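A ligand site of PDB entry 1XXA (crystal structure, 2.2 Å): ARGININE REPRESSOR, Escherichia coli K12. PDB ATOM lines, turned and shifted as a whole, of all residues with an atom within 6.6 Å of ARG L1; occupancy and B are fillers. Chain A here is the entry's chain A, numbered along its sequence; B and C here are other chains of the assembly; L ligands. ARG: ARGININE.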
ATOM      1  N   ALA A  27      -8.433   0.025  27.511  1.00  0.00           N
ATOM      2  CA  ALA A  27      -9.107   1.070  26.725  1.00  0.00           C
ATOM      3  C   ALA A  27      -9.899   2.093  27.538  1.00  0.00           C
ATOM      4  O   ALA A  27      -9.741   3.299  27.311  1.00  0.00           O
ATOM      5  CB  ALA A  27      -9.982   0.464  25.655  1.00  0.00           C
ATOM      6  N   GLN A  28     -10.718   1.653  28.481  1.00  0.00           N
ATOM      7  CA  GLN A  28     -11.498   2.633  29.263  1.00  0.00           C
ATOM      8  C   GLN A  28     -10.637   3.501  30.194  1.00  0.00           C
ATOM      9  O   GLN A  28     -10.906   4.703  30.366  1.00  0.00           O
ATOM     10  CB  GLN A  28     -12.649   1.937  30.021  1.00  0.00           C
ATOM     11  CG  GLN A  28     -13.828   1.495  29.134  1.00  0.00           C
ATOM     12  CD  GLN A  28     -14.794   2.629  28.803  1.00  0.00           C
ATOM     13  OE1 GLN A  28     -14.863   3.621  29.509  1.00  0.00           O
ATOM     14  NE2 GLN A  28     -15.596   2.446  27.757  1.00  0.00           N
ATOM     15  N   LEU A  29      -9.566   2.907  30.735  1.00  0.00           N
ATOM     16  CA  LEU A  29      -8.620   3.567  31.657  1.00  0.00           C
ATOM     17  C   LEU A  29      -7.858   4.663  30.904  1.00  0.00           C
ATOM     18  O   LEU A  29      -7.829   5.828  31.312  1.00  0.00           O
ATOM     19  CB  LEU A  29      -7.621   2.534  32.181  1.00  0.00           C
ATOM     20  CG  LEU A  29      -6.940   2.623  33.543  1.00  0.00           C
ATOM     21  CD1 LEU A  29      -5.647   1.820  33.441  1.00  0.00           C
ATOM     22  CD2 LEU A  29      -6.634   4.045  33.969  1.00  0.00           C
ATOM     23  N   ALA A  31      -8.666   5.847  28.060  1.00  0.00           N
ATOM     24  CA  ALA A  31      -9.670   6.786  27.582  1.00  0.00           C
ATOM     25  C   ALA A  31     -10.113   7.763  28.665  1.00  0.00           C
ATOM     26  O   ALA A  31     -10.473   8.905  28.368  1.00  0.00           O
ATOM     27  CB  ALA A  31     -10.869   6.056  27.033  1.00  0.00           C
ATOM     28  N   ARG A  32     -10.092   7.327  29.913  1.00  0.00           N
ATOM     29  CA  ARG A  32     -10.485   8.215  30.994  1.00  0.00           C
ATOM     30  C   ARG A  32      -9.457   9.343  31.076  1.00  0.00           C
ATOM     31  O   ARG A  32      -9.782  10.439  31.535  1.00  0.00           O
ATOM     32  CB  ARG A  32     -10.610   7.479  32.312  1.00  0.00           C
ATOM     33  CG  ARG A  32     -11.395   8.294  33.313  1.00  0.00           C
ATOM     34  CD  ARG A  32     -11.902   7.473  34.463  1.00  0.00           C
ATOM     35  NE  ARG A  32     -11.131   7.706  35.679  1.00  0.00           N
ATOM     36  CZ  ARG A  32     -10.052   7.001  36.024  1.00  0.00           C
ATOM     37  NH1 ARG A  32      -9.615   6.020  35.242  1.00  0.00           N
ATOM     38  NH2 ARG A  32      -9.453   7.252  37.175  1.00  0.00           N
ATOM     39  N   LEU A  33      -8.254   9.080  30.585  1.00  0.00           N
ATOM     40  CA  LEU A  33      -7.167  10.061  30.563  1.00  0.00           C
ATOM     41  C   LEU A  33      -7.516  11.181  29.567  1.00  0.00           C
ATOM     42  O   LEU A  33      -7.413  12.356  29.890  1.00  0.00           O
ATOM     43  CB  LEU A  33      -5.865   9.345  30.164  1.00  0.00           C
ATOM     44  CG  LEU A  33      -4.457   9.948  30.254  1.00  0.00           C
ATOM     45  CD1 LEU A  33      -3.427   8.852  29.985  1.00  0.00           C
ATOM     46  CD2 LEU A  33      -4.281  11.075  29.258  1.00  0.00           C
ATOM     47  N   ASP A  35     -10.382  12.224  28.700  1.00  0.00           N
ATOM     48  CA  ASP A  35     -11.519  13.021  29.149  1.00  0.00           C
ATOM     49  C   ASP A  35     -11.066  14.128  30.104  1.00  0.00           C
ATOM     50  O   ASP A  35     -11.872  14.928  30.562  1.00  0.00           O
ATOM     51  CB  ASP A  35     -12.577  12.122  29.826  1.00  0.00           C
ATOM     52  CG  ASP A  35     -13.239  11.150  28.843  1.00  0.00           C
ATOM     53  OD1 ASP A  35     -13.481  11.547  27.683  1.00  0.00           O
ATOM     54  OD2 ASP A  35     -13.523   9.995  29.246  1.00  0.00           O
ATOM     55  N   GLY A  45     -14.743  14.640  21.910  1.00  0.00           N
ATOM     56  CA  GLY A  45     -15.216  13.492  22.631  1.00  0.00           C
ATOM     57  C   GLY A  45     -14.392  12.266  22.306  1.00  0.00           C
ATOM     58  O   GLY A  45     -13.634  12.244  21.330  1.00  0.00           O
ATOM     59  N   THR A  46     -14.558  11.247  23.143  1.00  0.00           N
ATOM     60  CA  THR A  46     -13.842  10.003  22.988  1.00  0.00           C
ATOM     61  C   THR A  46     -14.682   8.828  23.531  1.00  0.00           C
ATOM     62  O   THR A  46     -15.392   8.987  24.530  1.00  0.00           O
ATOM     63  CB  THR A  46     -12.384  10.136  23.607  1.00  0.00           C
ATOM     64  OG1 THR A  46     -11.972   8.915  24.241  1.00  0.00           O
ATOM     65  CG2 THR A  46     -12.306  11.291  24.601  1.00  0.00           C
ATOM     66  N   ILE A  47     -14.741   7.752  22.741  1.00  0.00           N
ATOM     67  CA  ILE A  47     -15.437   6.511  23.064  1.00  0.00           C
ATOM     68  C   ILE A  47     -14.400   5.404  23.043  1.00  0.00           C
ATOM     69  O   ILE A  47     -13.548   5.354  22.140  1.00  0.00           O
ATOM     70  CB  ILE A  47     -16.511   6.102  22.033  1.00  0.00           C
ATOM     71  CG1 ILE A  47     -15.931   6.208  20.613  1.00  0.00           C
ATOM     72  CG2 ILE A  47     -17.790   6.918  22.198  1.00  0.00           C
ATOM     73  CD1 ILE A  47     -16.832   5.658  19.565  1.00  0.00           C
ATOM     74  N   ALA A  48     -14.462   4.516  24.028  1.00  0.00           N
ATOM     75  CA  ALA A  48     -13.515   3.446  24.091  1.00  0.00           C
ATOM     76  C   ALA A  48     -14.218   2.118  24.005  1.00  0.00           C
ATOM     77  O   ALA A  48     -15.371   1.994  24.409  1.00  0.00           O
ATOM     78  CB  ALA A  48     -12.751   3.525  25.375  1.00  0.00           C
ATOM     79  N   GLY A  49     -13.525   1.128  23.478  1.00  0.00           N
ATOM     80  CA  GLY A  49     -14.105  -0.193  23.386  1.00  0.00           C
ATOM     81  C   GLY A  49     -13.393  -1.069  24.399  1.00  0.00           C
ATOM     82  O   GLY A  49     -13.352  -0.744  25.577  1.00  0.00           O
ATOM     83  N   HIS B  21     -22.472  13.869  25.575  1.00  0.00           N
ATOM     84  CA  HIS B  21     -21.791  13.523  26.801  1.00  0.00           C
ATOM     85  C   HIS B  21     -22.893  13.320  27.803  1.00  0.00           C
ATOM     86  O   HIS B  21     -23.744  14.193  27.955  1.00  0.00           O
ATOM     87  CB  HIS B  21     -20.825  14.641  27.242  1.00  0.00           C
ATOM     88  CG  HIS B  21     -19.663  14.838  26.310  1.00  0.00           C
ATOM     89  ND1 HIS B  21     -19.681  15.785  25.299  1.00  0.00           N
ATOM     90  CD2 HIS B  21     -18.463  14.201  26.287  1.00  0.00           C
ATOM     91  CE1 HIS B  21     -18.520  15.703  24.691  1.00  0.00           C
ATOM     92  NE2 HIS B  21     -17.735  14.749  25.255  1.00  0.00           N
ATOM     93  N   PRO B  24     -22.102   9.520  33.925  1.00  0.00           N
ATOM     94  CA  PRO B  24     -21.403   8.240  33.840  1.00  0.00           C
ATOM     95  C   PRO B  24     -22.351   7.050  33.891  1.00  0.00           C
ATOM     96  O   PRO B  24     -23.286   7.027  34.682  1.00  0.00           O
ATOM     97  CB  PRO B  24     -20.459   8.293  35.037  1.00  0.00           C
ATOM     98  CG  PRO B  24     -21.070   9.276  35.922  1.00  0.00           C
ATOM     99  CD  PRO B  24     -21.562  10.328  35.006  1.00  0.00           C
ATOM    100  N   GLY B  25     -22.162   6.123  32.958  1.00  0.00           N
ATOM    101  CA  GLY B  25     -22.984   4.932  32.914  1.00  0.00           C
ATOM    102  C   GLY B  25     -24.287   5.127  32.181  1.00  0.00           C
ATOM    103  O   GLY B  25     -25.033   4.174  32.017  1.00  0.00           O
ATOM    104  N   ALA B  27     -24.550   6.200  28.936  1.00  0.00           N
ATOM    105  CA  ALA B  27     -24.378   6.158  27.484  1.00  0.00           C
ATOM    106  C   ALA B  27     -25.233   5.136  26.734  1.00  0.00           C
ATOM    107  O   ALA B  27     -25.945   5.492  25.786  1.00  0.00           O
ATOM    108  CB  ALA B  27     -22.932   5.942  27.120  1.00  0.00           C
ATOM    109  N   ALA B  48     -22.020   3.789  21.890  1.00  0.00           N
ATOM    110  CA  ALA B  48     -21.914   4.320  23.239  1.00  0.00           C
ATOM    111  C   ALA B  48     -20.822   3.666  24.060  1.00  0.00           C
ATOM    112  O   ALA B  48     -20.554   2.471  23.956  1.00  0.00           O
ATOM    113  CB  ALA B  48     -23.246   4.144  23.967  1.00  0.00           C
ATOM    114  N   GLY B  49     -20.198   4.480  24.896  1.00  0.00           N
ATOM    115  CA  GLY B  49     -19.162   4.009  25.770  1.00  0.00           C
ATOM    116  C   GLY B  49     -19.827   4.062  27.118  1.00  0.00           C
ATOM    117  O   GLY B  49     -20.928   3.550  27.274  1.00  0.00           O
ATOM    118  N   ASP B  50     -19.191   4.740  28.066  1.00  0.00           N
ATOM    119  CA  ASP B  50     -19.728   4.866  29.419  1.00  0.00           C
ATOM    120  C   ASP B  50     -20.379   6.221  29.629  1.00  0.00           C
ATOM    121  O   ASP B  50     -21.441   6.312  30.257  1.00  0.00           O
ATOM    122  CB  ASP B  50     -18.619   4.646  30.437  1.00  0.00           C
ATOM    123  CG  ASP B  50     -19.142   4.461  31.848  1.00  0.00           C
ATOM    124  OD1 ASP B  50     -19.523   3.330  32.188  1.00  0.00           O
ATOM    125  OD2 ASP B  50     -19.163   5.428  32.625  1.00  0.00           O
ATOM    126  N   ASP B  51     -19.765   7.279  29.082  1.00  0.00           N
ATOM    127  CA  ASP B  51     -20.293   8.629  29.205  1.00  0.00           C
ATOM    128  C   ASP B  51     -20.341   9.392  27.911  1.00  0.00           C
ATOM    129  O   ASP B  51     -20.741  10.548  27.890  1.00  0.00           O
ATOM    130  CB  ASP B  51     -19.474   9.455  30.198  1.00  0.00           C
ATOM    131  CG  ASP B  51     -17.998   9.517  29.844  1.00  0.00           C
ATOM    132  OD1 ASP B  51     -17.629   9.193  28.717  1.00  0.00           O
ATOM    133  OD2 ASP B  51     -17.200   9.897  30.722  1.00  0.00           O
ATOM    134  N   THR B  52     -19.863   8.759  26.848  1.00  0.00           N
ATOM    135  CA  THR B  52     -19.847   9.394  25.532  1.00  0.00           C
ATOM    136  C   THR B  52     -20.531   8.547  24.474  1.00  0.00           C
ATOM    137  O   THR B  52     -20.446   7.323  24.493  1.00  0.00           O
ATOM    138  CB  THR B  52     -18.419   9.625  25.044  1.00  0.00           C
ATOM    139  OG1 THR B  52     -17.591  10.008  26.138  1.00  0.00           O
ATOM    140  CG2 THR B  52     -18.386  10.704  23.981  1.00  0.00           C
ATOM    141  N   ILE B  53     -21.157   9.208  23.515  1.00  0.00           N
ATOM    142  CA  ILE B  53     -21.836   8.535  22.426  1.00  0.00           C
ATOM    143  C   ILE B  53     -21.416   9.236  21.137  1.00  0.00           C
ATOM    144  O   ILE B  53     -21.383  10.458  21.107  1.00  0.00           O
ATOM    145  CB  ILE B  53     -23.357   8.675  22.570  1.00  0.00           C
ATOM    146  CG1 ILE B  53     -23.813   8.075  23.903  1.00  0.00           C
ATOM    147  CG2 ILE B  53     -24.031   8.033  21.384  1.00  0.00           C
ATOM    148  CD1 ILE B  53     -25.196   8.435  24.307  1.00  0.00           C
ATOM    149  N   PRO C  24     -12.172   4.127  38.395  1.00  0.00           N
ATOM    150  CA  PRO C  24     -13.165   4.087  37.307  1.00  0.00           C
ATOM    151  C   PRO C  24     -12.539   3.544  36.011  1.00  0.00           C
ATOM    152  O   PRO C  24     -11.415   3.878  35.675  1.00  0.00           O
ATOM    153  CB  PRO C  24     -13.550   5.554  37.171  1.00  0.00           C
ATOM    154  CG  PRO C  24     -13.507   6.029  38.582  1.00  0.00           C
ATOM    155  CD  PRO C  24     -12.247   5.415  39.116  1.00  0.00           C
ATOM    156  N   GLY C  25     -13.227   2.615  35.360  1.00  0.00           N
ATOM    157  CA  GLY C  25     -12.725   2.070  34.114  1.00  0.00           C
ATOM    158  C   GLY C  25     -11.502   1.161  34.187  1.00  0.00           C
ATOM    159  O   GLY C  25     -11.053   0.655  33.156  1.00  0.00           O
ATOM    160  N   ALA C  26     -10.990   0.920  35.397  1.00  0.00           N
ATOM    161  CA  ALA C  26      -9.813   0.065  35.571  1.00  0.00           C
ATOM    162  C   ALA C  26     -10.139  -1.415  35.762  1.00  0.00           C
ATOM    163  O   ALA C  26      -9.280  -2.280  35.582  1.00  0.00           O
ATOM    164  CB  ALA C  26      -8.972   0.572  36.730  1.00  0.00           C
ATOM    165  N   ASP C  50     -17.315  -1.830  35.666  1.00  0.00           N
ATOM    166  CA  ASP C  50     -16.525  -0.649  35.328  1.00  0.00           C
ATOM    167  C   ASP C  50     -15.466  -0.284  36.363  1.00  0.00           C
ATOM    168  O   ASP C  50     -14.435   0.277  36.007  1.00  0.00           O
ATOM    169  CB  ASP C  50     -17.393   0.578  35.077  1.00  0.00           C
ATOM    170  CG  ASP C  50     -16.566   1.787  34.661  1.00  0.00           C
ATOM    171  OD1 ASP C  50     -16.119   1.830  33.509  1.00  0.00           O
ATOM    172  OD2 ASP C  50     -16.345   2.710  35.470  1.00  0.00           O
HETATM  173  N   ARG L   1     -15.461   8.533  27.333  1.00  0.00           N
HETATM  174  CA  ARG L   1     -15.035   7.126  27.164  1.00  0.00           C
HETATM  175  C   ARG L   1     -16.289   6.324  26.859  1.00  0.00           C
HETATM  176  O   ARG L   1     -16.128   5.186  26.372  1.00  0.00           O
HETATM  177  CB  ARG L   1     -14.325   6.622  28.423  1.00  0.00           C
HETATM  178  CG  ARG L   1     -15.007   6.927  29.737  1.00  0.00           C
HETATM  179  CD  ARG L   1     -14.080   6.569  30.898  1.00  0.00           C
HETATM  180  NE  ARG L   1     -14.813   6.268  32.127  1.00  0.00           N
HETATM  181  CZ  ARG L   1     -15.088   5.036  32.573  1.00  0.00           C
HETATM  182  NH1 ARG L   1     -14.681   3.981  31.879  1.00  0.00           N
HETATM  183  NH2 ARG L   1     -15.762   4.853  33.693  1.00  0.00           N
HETATM  184  OXT ARG L   1     -17.409   6.867  27.059  1.00  0.00           O
HETATM  185  N   ARG L   2     -20.256  -0.756  40.306  1.00  0.00           N
HETATM  186  CA  ARG L   2     -20.850  -1.097  38.998  1.00  0.00           C
HETATM  187  C   ARG L   2     -19.791  -1.722  38.103  1.00  0.00           C
HETATM  188  O   ARG L   2     -20.117  -2.557  37.237  1.00  0.00           O
HETATM  189  CB  ARG L   2     -21.469   0.130  38.340  1.00  0.00           C
HETATM  190  CG  ARG L   2     -20.522   1.222  37.866  1.00  0.00           C
HETATM  191  CD  ARG L   2     -21.354   2.423  37.443  1.00  0.00           C
HETATM  192  NE  ARG L   2     -20.545   3.572  37.068  1.00  0.00           N
HETATM  193  CZ  ARG L   2     -20.131   3.815  35.828  1.00  0.00           C
HETATM  194  NH1 ARG L   2     -20.456   2.985  34.845  1.00  0.00           N
HETATM  195  NH2 ARG L   2     -19.390   4.889  35.562  1.00  0.00           N
HETATM  196  OXT ARG L   2     -18.607  -1.424  38.316  1.00  0.00           O
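NE2 of Gln 28 lies within hydrogen-bond range of O of Ala 48 of chain A (3.4 Å). OD1 of Asp 51 of chain B lies within hydrogen-bond range of OG1 of Thr 52 of chain B (2.7 Å). The side-chain hydroxyl (OG1) of Thr 52 of chain B is in hydrogen-bond range of the backbone carbonyl oxygen (O) of Thr 46 (2.9 Å). The backbone carbonyl oxygen of Asp 50 of chain C sits at hydrogen-bond distance from the backbone NH of Gly 25 of chain C (2.7 Å). O of Asp 50 of chain B is in hydrogen-bond range of N of Ala 27 of chain B (3.4 Å). The backbone carbonyl oxygen of Pro 24 of chain C is in hydrogen-bond range of the guanidinium group of Arg 32 (2.8 Å).
The side-chain amide oxygen (OE1) of Gln 28 lies within hydrogen-bond range of a nitrogen (NH1) of ARG L1. The backbone NH (N) of Asp 51 of chain B is in hydrogen-bond range of an oxygen (OXT) of ARG L1, 3.1 Å away. OD1 of Asp 51 of chain B is in salt-bridge range of N of ARG L1 (2.7 Å). The backbone carbonyl oxygen of Thr 46 is in hydrogen-bond range of a nitrogen (N) of ARG L1 (2.8 Å). A nitrogen (NH2) of ARG L1 lies within salt-bridge range of the side-chain carboxylate of Asp 50 of chain C (2.8 Å). N of Thr 52 of chain B is in hydrogen-bond range of OXT of ARG L1, 3.1 Å away. The side-chain hydroxyl (OG1) of Thr 52 of chain B lies within hydrogen-bond range of a nitrogen (N) of ARG L1, at 2.9 Å. The backbone NH (N) of Asp 50 of chain B sits at hydrogen-bond distance from an oxygen (OXT) of ARG L1 (3.0 Å). The side-chain carboxylate of Asp 50 of chain B lies within salt-bridge range of a nitrogen (NH2) of ARG L1 (3.6 Å). The backbone NH (N) of Ala 48 of chain A sits at hydrogen-bond distance from an oxygen (O) of ARG L1, at 3.0 Å. OD2 of Asp 35 is in salt-bridge range of N of ARG L1. The backbone NH (N) of Asp 50 of chain C is in hydrogen-bond range of an oxygen (OXT) of ARG L2, 3.0 Å away. The side-chain carboxylate (OD2) of Asp 50 of chain C lies within salt-bridge range of a nitrogen (NH2) of ARG L2 (3.7 Å). The side-chain carboxylate of Asp 50 of chain B lies within salt-bridge range of a nitrogen (NH1) of ARG L2, 2.8 Å away.
Merely in contact with ARG L1: Ala 31 (3.8 Å), Arg 32 (3.9 Å), Ile 47 (3.6 Å), Gly 49 of chain B (3.3 Å) and Gly 25 of chain C (3.5 Å). Hydrophobic or aromatic side chains that line ARG L1: Ala 31 and Ala 48 of chain A. Within 4 Å of ARG L1: Gln 28, Ala 31, Arg 32, Asp 35, Thr 46, Ile 47, Ala 48 of chain A, Gly 49 of chain B, Asp 50 of chain B, Asp 51 of chain B, Thr 52 of chain B, Gly 25 of chain C and Asp 50 of chain C. The nearest printed residue that does not touch ARG L1 is Pro 24 of chain C (4.2 Å).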
